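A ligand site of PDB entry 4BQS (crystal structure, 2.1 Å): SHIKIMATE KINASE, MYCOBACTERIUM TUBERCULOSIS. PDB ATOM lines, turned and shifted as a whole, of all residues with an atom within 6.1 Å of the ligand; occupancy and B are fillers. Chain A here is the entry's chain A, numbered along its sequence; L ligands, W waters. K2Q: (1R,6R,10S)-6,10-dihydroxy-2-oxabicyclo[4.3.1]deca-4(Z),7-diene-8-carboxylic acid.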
ATOM      1  N   LEU A  10     -22.357 -15.879  19.649  1.00  0.00           N
ATOM      2  CA  LEU A  10     -22.440 -15.167  20.888  1.00  0.00           C
ATOM      3  C   LEU A  10     -23.900 -15.041  21.302  1.00  0.00           C
ATOM      4  O   LEU A  10     -24.810 -15.228  20.484  1.00  0.00           O
ATOM      5  CB  LEU A  10     -21.852 -13.771  20.726  1.00  0.00           C
ATOM      6  CG  LEU A  10     -20.361 -13.701  20.381  1.00  0.00           C
ATOM      7  CD1 LEU A  10     -20.134 -12.337  19.802  1.00  0.00           C
ATOM      8  CD2 LEU A  10     -19.492 -13.946  21.591  1.00  0.00           C
ATOM      9  N   PRO A  11     -24.125 -14.709  22.581  1.00  0.00           N
ATOM     10  CA  PRO A  11     -25.456 -14.439  23.054  1.00  0.00           C
ATOM     11  C   PRO A  11     -25.950 -13.242  22.295  1.00  0.00           C
ATOM     12  O   PRO A  11     -25.159 -12.393  21.941  1.00  0.00           O
ATOM     13  CB  PRO A  11     -25.273 -14.137  24.532  1.00  0.00           C
ATOM     14  CG  PRO A  11     -23.823 -13.913  24.745  1.00  0.00           C
ATOM     15  CD  PRO A  11     -23.093 -14.571  23.638  1.00  0.00           C
ATOM     16  N   LYS A  15     -29.680 -17.609  18.606  1.00  0.00           N
ATOM     17  CA  LYS A  15     -29.659 -19.051  18.618  1.00  0.00           C
ATOM     18  C   LYS A  15     -30.986 -19.680  19.024  1.00  0.00           C
ATOM     19  O   LYS A  15     -31.338 -20.708  18.487  1.00  0.00           O
ATOM     20  CB  LYS A  15     -28.556 -19.598  19.506  1.00  0.00           C
ATOM     21  CG  LYS A  15     -27.169 -19.132  19.093  1.00  0.00           C
ATOM     22  CD  LYS A  15     -26.094 -19.873  19.842  1.00  0.00           C
ATOM     23  CE  LYS A  15     -26.073 -19.485  21.325  1.00  0.00           C
ATOM     24  NZ  LYS A  15     -25.709 -18.071  21.572  1.00  0.00           N
ATOM     25  N   ASP A  34     -27.287 -25.027  27.041  1.00  0.00           N
ATOM     26  CA  ASP A  34     -27.502 -24.297  28.272  1.00  0.00           C
ATOM     27  C   ASP A  34     -28.633 -24.884  29.145  1.00  0.00           C
ATOM     28  O   ASP A  34     -28.475 -25.123  30.347  1.00  0.00           O
ATOM     29  CB  ASP A  34     -27.780 -22.833  27.985  1.00  0.00           C
ATOM     30  CG  ASP A  34     -26.509 -22.015  27.698  1.00  0.00           C
ATOM     31  OD1 ASP A  34     -25.366 -22.490  27.904  1.00  0.00           O
ATOM     32  OD2 ASP A  34     -26.663 -20.894  27.208  1.00  0.00           O
ATOM     33  N   ILE A  37     -27.617 -28.310  30.317  1.00  0.00           N
ATOM     34  CA  ILE A  37     -26.753 -28.240  31.523  1.00  0.00           C
ATOM     35  C   ILE A  37     -27.584 -28.125  32.799  1.00  0.00           C
ATOM     36  O   ILE A  37     -27.322 -28.782  33.791  1.00  0.00           O
ATOM     37  CB  ILE A  37     -25.735 -27.067  31.444  1.00  0.00           C
ATOM     38  CG1 ILE A  37     -24.639 -27.427  30.426  1.00  0.00           C
ATOM     39  CG2 ILE A  37     -25.094 -26.765  32.786  1.00  0.00           C
ATOM     40  CD1 ILE A  37     -23.894 -26.218  29.907  1.00  0.00           C
ATOM     41  N   ILE A  45     -27.291 -21.835  35.565  1.00  0.00           N
ATOM     42  CA  ILE A  45     -26.001 -21.558  35.020  1.00  0.00           C
ATOM     43  C   ILE A  45     -25.265 -20.566  35.899  1.00  0.00           C
ATOM     44  O   ILE A  45     -24.079 -20.804  36.221  1.00  0.00           O
ATOM     45  CB  ILE A  45     -26.049 -21.140  33.550  1.00  0.00           C
ATOM     46  CG1 ILE A  45     -26.486 -22.368  32.723  1.00  0.00           C
ATOM     47  CG2 ILE A  45     -24.680 -20.636  33.118  1.00  0.00           C
ATOM     48  CD1 ILE A  45     -26.585 -22.114  31.250  1.00  0.00           C
ATOM     49  N   PHE A  49     -21.349 -20.983  37.745  1.00  0.00           N
ATOM     50  CA  PHE A  49     -20.289 -19.974  37.607  1.00  0.00           C
ATOM     51  C   PHE A  49     -19.868 -19.400  38.955  1.00  0.00           C
ATOM     52  O   PHE A  49     -18.671 -19.475  39.343  1.00  0.00           O
ATOM     53  CB  PHE A  49     -20.687 -18.799  36.687  1.00  0.00           C
ATOM     54  CG  PHE A  49     -20.382 -19.041  35.239  1.00  0.00           C
ATOM     55  CD1 PHE A  49     -21.231 -19.791  34.452  1.00  0.00           C
ATOM     56  CD2 PHE A  49     -19.199 -18.572  34.682  1.00  0.00           C
ATOM     57  CE1 PHE A  49     -20.945 -20.012  33.111  1.00  0.00           C
ATOM     58  CE2 PHE A  49     -18.906 -18.792  33.349  1.00  0.00           C
ATOM     59  CZ  PHE A  49     -19.772 -19.508  32.556  1.00  0.00           C
ATOM     60  N   GLU A  54     -15.799 -20.989  36.274  1.00  0.00           N
ATOM     61  CA  GLU A  54     -16.089 -21.172  34.854  1.00  0.00           C
ATOM     62  C   GLU A  54     -15.452 -22.453  34.344  1.00  0.00           C
ATOM     63  O   GLU A  54     -16.074 -23.198  33.599  1.00  0.00           O
ATOM     64  CB  GLU A  54     -15.607 -19.982  34.018  1.00  0.00           C
ATOM     65  CG  GLU A  54     -15.562 -20.282  32.541  1.00  0.00           C
ATOM     66  CD  GLU A  54     -15.319 -19.083  31.671  1.00  0.00           C
ATOM     67  OE1 GLU A  54     -15.089 -17.944  32.185  1.00  0.00           O
ATOM     68  OE2 GLU A  54     -15.379 -19.299  30.432  1.00  0.00           O
ATOM     69  N   PHE A  57     -17.688 -25.107  35.011  1.00  0.00           N
ATOM     70  CA  PHE A  57     -18.756 -24.979  34.026  1.00  0.00           C
ATOM     71  C   PHE A  57     -18.365 -25.526  32.644  1.00  0.00           C
ATOM     72  O   PHE A  57     -19.111 -26.284  32.024  1.00  0.00           O
ATOM     73  CB  PHE A  57     -19.231 -23.528  33.901  1.00  0.00           C
ATOM     74  CG  PHE A  57     -20.334 -23.335  32.881  1.00  0.00           C
ATOM     75  CD1 PHE A  57     -21.629 -23.661  33.185  1.00  0.00           C
ATOM     76  CD2 PHE A  57     -20.042 -22.920  31.611  1.00  0.00           C
ATOM     77  CE1 PHE A  57     -22.634 -23.512  32.262  1.00  0.00           C
ATOM     78  CE2 PHE A  57     -21.050 -22.781  30.652  1.00  0.00           C
ATOM     79  CZ  PHE A  57     -22.352 -23.070  30.982  1.00  0.00           C
ATOM     80  N   ARG A  58     -17.185 -25.167  32.139  1.00  0.00           N
ATOM     81  CA  ARG A  58     -16.787 -25.631  30.801  1.00  0.00           C
ATOM     82  C   ARG A  58     -16.695 -27.145  30.697  1.00  0.00           C
ATOM     83  O   ARG A  58     -16.854 -27.714  29.589  1.00  0.00           O
ATOM     84  CB  ARG A  58     -15.423 -25.031  30.328  1.00  0.00           C
ATOM     85  CG  ARG A  58     -15.384 -23.514  30.261  1.00  0.00           C
ATOM     86  CD  ARG A  58     -16.385 -23.015  29.239  1.00  0.00           C
ATOM     87  NE  ARG A  58     -16.564 -21.561  29.284  1.00  0.00           N
ATOM     88  CZ  ARG A  58     -17.679 -20.941  28.864  1.00  0.00           C
ATOM     89  NH1 ARG A  58     -18.715 -21.621  28.361  1.00  0.00           N
ATOM     90  NH2 ARG A  58     -17.795 -19.617  28.972  1.00  0.00           N
ATOM     91  N   GLU A  61     -20.226 -28.482  30.491  1.00  0.00           N
ATOM     92  CA  GLU A  61     -20.674 -28.113  29.155  1.00  0.00           C
ATOM     93  C   GLU A  61     -20.106 -29.045  28.124  1.00  0.00           C
ATOM     94  O   GLU A  61     -20.795 -29.478  27.187  1.00  0.00           O
ATOM     95  CB  GLU A  61     -20.254 -26.661  28.819  1.00  0.00           C
ATOM     96  CG  GLU A  61     -20.681 -26.133  27.474  1.00  0.00           C
ATOM     97  CD  GLU A  61     -20.363 -24.660  27.291  1.00  0.00           C
ATOM     98  OE1 GLU A  61     -19.170 -24.253  27.453  1.00  0.00           O
ATOM     99  OE2 GLU A  61     -21.299 -23.896  26.954  1.00  0.00           O
ATOM    100  N   LEU A  78     -25.417 -24.446  20.760  1.00  0.00           N
ATOM    101  CA  LEU A  78     -24.444 -24.387  21.832  1.00  0.00           C
ATOM    102  C   LEU A  78     -24.439 -23.040  22.544  1.00  0.00           C
ATOM    103  O   LEU A  78     -24.650 -21.967  21.923  1.00  0.00           O
ATOM    104  CB  LEU A  78     -23.031 -24.630  21.293  1.00  0.00           C
ATOM    105  CG  LEU A  78     -22.745 -25.784  20.367  1.00  0.00           C
ATOM    106  CD1 LEU A  78     -21.236 -25.892  20.190  1.00  0.00           C
ATOM    107  CD2 LEU A  78     -23.317 -27.062  20.896  1.00  0.00           C
ATOM    108  N   GLY A  79     -24.125 -23.072  23.837  1.00  0.00           N
ATOM    109  CA  GLY A  79     -23.924 -21.862  24.579  1.00  0.00           C
ATOM    110  C   GLY A  79     -22.776 -21.108  23.969  1.00  0.00           C
ATOM    111  O   GLY A  79     -21.858 -21.741  23.393  1.00  0.00           O
ATOM    112  N   GLY A  80     -22.807 -19.780  24.151  1.00  0.00           N
ATOM    113  CA  GLY A  80     -21.863 -18.853  23.538  1.00  0.00           C
ATOM    114  C   GLY A  80     -20.388 -19.190  23.679  1.00  0.00           C
ATOM    115  O   GLY A  80     -19.598 -18.909  22.765  1.00  0.00           O
ATOM    116  N   GLY A  81     -19.977 -19.827  24.765  1.00  0.00           N
ATOM    117  CA  GLY A  81     -18.532 -20.016  25.010  1.00  0.00           C
ATOM    118  C   GLY A  81     -18.021 -21.437  24.828  1.00  0.00           C
ATOM    119  O   GLY A  81     -16.837 -21.717  25.093  1.00  0.00           O
ATOM    120  N   ALA A  82     -18.925 -22.335  24.415  1.00  0.00           N
ATOM    121  CA  ALA A  82     -18.629 -23.728  24.228  1.00  0.00           C
ATOM    122  C   ALA A  82     -17.438 -23.918  23.296  1.00  0.00           C
ATOM    123  O   ALA A  82     -16.600 -24.723  23.553  1.00  0.00           O
ATOM    124  CB  ALA A  82     -19.840 -24.422  23.655  1.00  0.00           C
ATOM    125  N   THR A 115     -31.669 -10.670  31.818  1.00  0.00           N
ATOM    126  CA  THR A 115     -31.059 -11.974  31.862  1.00  0.00           C
ATOM    127  C   THR A 115     -29.688 -11.939  32.601  1.00  0.00           C
ATOM    128  O   THR A 115     -28.877 -11.014  32.444  1.00  0.00           O
ATOM    129  CB  THR A 115     -30.850 -12.371  30.423  1.00  0.00           C
ATOM    130  OG1 THR A 115     -31.948 -11.803  29.700  1.00  0.00           O
ATOM    131  CG2 THR A 115     -30.810 -13.842  30.221  1.00  0.00           C
ATOM    132  N   VAL A 116     -29.462 -12.936  33.435  1.00  0.00           N
ATOM    133  CA  VAL A 116     -28.231 -13.076  34.197  1.00  0.00           C
ATOM    134  C   VAL A 116     -27.180 -13.649  33.263  1.00  0.00           C
ATOM    135  O   VAL A 116     -27.404 -14.686  32.668  1.00  0.00           O
ATOM    136  CB  VAL A 116     -28.421 -14.063  35.384  1.00  0.00           C
ATOM    137  CG1 VAL A 116     -27.088 -14.354  36.059  1.00  0.00           C
ATOM    138  CG2 VAL A 116     -29.441 -13.496  36.373  1.00  0.00           C
ATOM    139  N   ARG A 117     -26.062 -12.965  33.084  1.00  0.00           N
ATOM    140  CA  ARG A 117     -25.001 -13.521  32.258  1.00  0.00           C
ATOM    141  C   ARG A 117     -23.680 -13.294  32.976  1.00  0.00           C
ATOM    142  O   ARG A 117     -23.210 -12.157  33.078  1.00  0.00           O
ATOM    143  CB  ARG A 117     -24.989 -12.888  30.869  1.00  0.00           C
ATOM    144  CG  ARG A 117     -26.337 -12.955  30.143  1.00  0.00           C
ATOM    145  CD  ARG A 117     -26.132 -12.663  28.650  1.00  0.00           C
ATOM    146  NE  ARG A 117     -27.332 -12.905  27.897  1.00  0.00           N
ATOM    147  CZ  ARG A 117     -28.287 -12.019  27.674  1.00  0.00           C
ATOM    148  NH1 ARG A 117     -28.194 -10.775  28.126  1.00  0.00           N
ATOM    149  NH2 ARG A 117     -29.372 -12.395  27.020  1.00  0.00           N
ATOM    150  N   PRO A 118     -23.099 -14.370  33.500  1.00  0.00           N
ATOM    151  CA  PRO A 118     -21.867 -14.256  34.291  1.00  0.00           C
ATOM    152  C   PRO A 118     -20.772 -13.558  33.524  1.00  0.00           C
ATOM    153  O   PRO A 118     -20.086 -12.764  34.068  1.00  0.00           O
ATOM    154  CB  PRO A 118     -21.532 -15.720  34.664  1.00  0.00           C
ATOM    155  CG  PRO A 118     -22.871 -16.398  34.671  1.00  0.00           C
ATOM    156  CD  PRO A 118     -23.725 -15.688  33.626  1.00  0.00           C
ATOM    157  N   LEU A 119     -20.614 -13.820  32.249  1.00  0.00           N
ATOM    158  CA  LEU A 119     -19.568 -13.169  31.508  1.00  0.00           C
ATOM    159  C   LEU A 119     -20.076 -11.937  30.768  1.00  0.00           C
ATOM    160  O   LEU A 119     -19.384 -11.417  29.878  1.00  0.00           O
ATOM    161  CB  LEU A 119     -18.890 -14.147  30.524  1.00  0.00           C
ATOM    162  CG  LEU A 119     -18.440 -15.477  31.119  1.00  0.00           C
ATOM    163  CD1 LEU A 119     -17.799 -16.420  30.094  1.00  0.00           C
ATOM    164  CD2 LEU A 119     -17.506 -15.217  32.266  1.00  0.00           C
ATOM    165  N   LEU A 132     -15.324 -10.585  23.908  1.00  0.00           N
ATOM    166  CA  LEU A 132     -15.835 -11.924  23.586  1.00  0.00           C
ATOM    167  C   LEU A 132     -15.813 -12.201  22.085  1.00  0.00           C
ATOM    168  O   LEU A 132     -15.399 -13.261  21.660  1.00  0.00           O
ATOM    169  CB  LEU A 132     -17.278 -12.122  24.116  1.00  0.00           C
ATOM    170  CG  LEU A 132     -17.408 -12.203  25.622  1.00  0.00           C
ATOM    171  CD1 LEU A 132     -18.835 -12.582  25.932  1.00  0.00           C
ATOM    172  CD2 LEU A 132     -16.434 -13.205  26.229  1.00  0.00           C
ATOM    173  N   ARG A 136     -13.589 -14.889  20.251  1.00  0.00           N
ATOM    174  CA  ARG A 136     -14.320 -16.082  19.799  1.00  0.00           C
ATOM    175  C   ARG A 136     -14.668 -16.099  18.316  1.00  0.00           C
ATOM    176  O   ARG A 136     -14.925 -17.167  17.744  1.00  0.00           O
ATOM    177  CB  ARG A 136     -15.581 -16.216  20.642  1.00  0.00           C
ATOM    178  CG  ARG A 136     -15.300 -16.489  22.106  1.00  0.00           C
ATOM    179  CD  ARG A 136     -16.582 -16.440  22.863  1.00  0.00           C
ATOM    180  NE  ARG A 136     -16.468 -16.615  24.307  1.00  0.00           N
ATOM    181  CZ  ARG A 136     -17.510 -16.593  25.128  1.00  0.00           C
ATOM    182  NH1 ARG A 136     -18.759 -16.430  24.687  1.00  0.00           N
ATOM    183  NH2 ARG A 136     -17.325 -16.728  26.420  1.00  0.00           N
ATOM    184  N   TYR A 140     -15.421 -19.475  16.132  1.00  0.00           N
ATOM    185  CA  TYR A 140     -16.640 -19.763  15.376  1.00  0.00           C
ATOM    186  C   TYR A 140     -16.358 -19.990  13.892  1.00  0.00           C
ATOM    187  O   TYR A 140     -16.888 -20.918  13.290  1.00  0.00           O
ATOM    188  CB  TYR A 140     -17.670 -18.671  15.529  1.00  0.00           C
ATOM    189  CG  TYR A 140     -18.163 -18.422  16.926  1.00  0.00           C
ATOM    190  CD1 TYR A 140     -18.674 -19.446  17.742  1.00  0.00           C
ATOM    191  CD2 TYR A 140     -18.169 -17.144  17.419  1.00  0.00           C
ATOM    192  CE1 TYR A 140     -19.107 -19.169  19.039  1.00  0.00           C
ATOM    193  CE2 TYR A 140     -18.588 -16.875  18.679  1.00  0.00           C
ATOM    194  CZ  TYR A 140     -19.081 -17.863  19.485  1.00  0.00           C
ATOM    195  OH  TYR A 140     -19.513 -17.447  20.728  1.00  0.00           O
HETATM  196  OAA K2Q L   1     -19.598 -17.714  27.772  1.00  0.00           O
HETATM  197  CAK K2Q L   1     -20.762 -17.355  27.312  1.00  0.00           C
HETATM  198  OAB K2Q L   1     -20.827 -16.578  26.325  1.00  0.00           O
HETATM  199  CAL K2Q L   1     -21.943 -17.912  27.844  1.00  0.00           C
HETATM  200  CAI K2Q L   1     -21.781 -18.658  29.049  1.00  0.00           C
HETATM  201  CAG K2Q L   1     -23.235 -17.664  27.276  1.00  0.00           C
HETATM  202  CAO K2Q L   1     -24.428 -18.326  27.692  1.00  0.00           C
HETATM  203  OAD K2Q L   1     -24.859 -19.152  26.592  1.00  0.00           O
HETATM  204  CAF K2Q L   1     -25.436 -17.422  28.038  1.00  0.00           C
HETATM  205  CAE K2Q L   1     -25.799 -17.058  29.324  1.00  0.00           C
HETATM  206  CAH K2Q L   1     -25.139 -17.482  30.511  1.00  0.00           C
HETATM  207  OAJ K2Q L   1     -23.677 -17.561  30.315  1.00  0.00           O
HETATM  208  CAN K2Q L   1     -23.168 -18.825  29.780  1.00  0.00           C
HETATM  209  CAM K2Q L   1     -24.155 -19.420  28.827  1.00  0.00           C
HETATM  210  OAC K2Q L   1     -23.573 -20.650  28.249  1.00  0.00           O
HETATM  211  O   HOH W   1     -21.638 -14.152  27.651  1.00  0.00           O
HETATM  212  O   HOH W   2     -22.555 -15.093  30.237  1.00  0.00           O
HETATM  213  O   HOH W   3     -21.224 -21.218  26.855  1.00  0.00           O
HETATM  214  O   HOH W   4     -25.597 -17.650  24.274  1.00  0.00           O
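Water W2 bridges an oxygen (OAJ) of the ligand (2.7 Å) and the backbone NH (N) of Leu 119 (3.1 Å). Water W4 bridges NZ of Lys 15 (2.7 Å) and OAD of the ligand (2.9 Å).
NH2 of Arg 58 lies within salt-bridge range of OAA of the ligand (2.9 Å). NH1 of Arg 136 lies within salt-bridge range of OAB of the ligand (2.6 Å). An oxygen (OAD) of the ligand sits at hydrogen-bond distance from the side-chain carboxylate (OD2) of Asp 34, at 2.6 Å. The backbone NH (N) of Gly 80 sits at hydrogen-bond distance from an oxygen (OAD) of the ligand (3.3 Å).
The guanidinium group (NH1) of Arg 136 sits at hydrogen-bond distance from the backbone carbonyl oxygen (O) of Gly 80, at 3.2 Å. The guanidinium group (NE) of Arg 58 is in salt-bridge range of the side-chain carboxylate (OE2) of Glu 54 (2.8 Å). NH1 of Arg 58 is in salt-bridge range of OE1 of Glu 61, 2.8 Å away. O of Gly 80 sits at hydrogen-bond distance from OH of Tyr 140, at 2.5 Å.
Phe 57 touches the ligand (CZ to OAC, 3.8 Å). CA of Gly 79 touches OAD of the ligand, 3.5 Å away. Gly 81 touches the ligand (N to CAK, 3.6 Å). Pro 118 touches the ligand. Leu 119 touches the ligand (CD1 to OAA, 3.2 Å). Hydrophobic or aromatic side chains that line the ligand: Phe 57, Pro 118 and Leu 119. Nine residues have an atom within 4 Å of the ligand: Asp 34, Phe 57, Arg 58, Gly 79, Gly 80, Gly 81, Pro 118, Leu 119 and Arg 136. Along chain A the residues within 4 Å of the ligand span positions 34 to 136. The nearest printed residue that does not touch the ligand is Pro 11 (4.05 Å).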
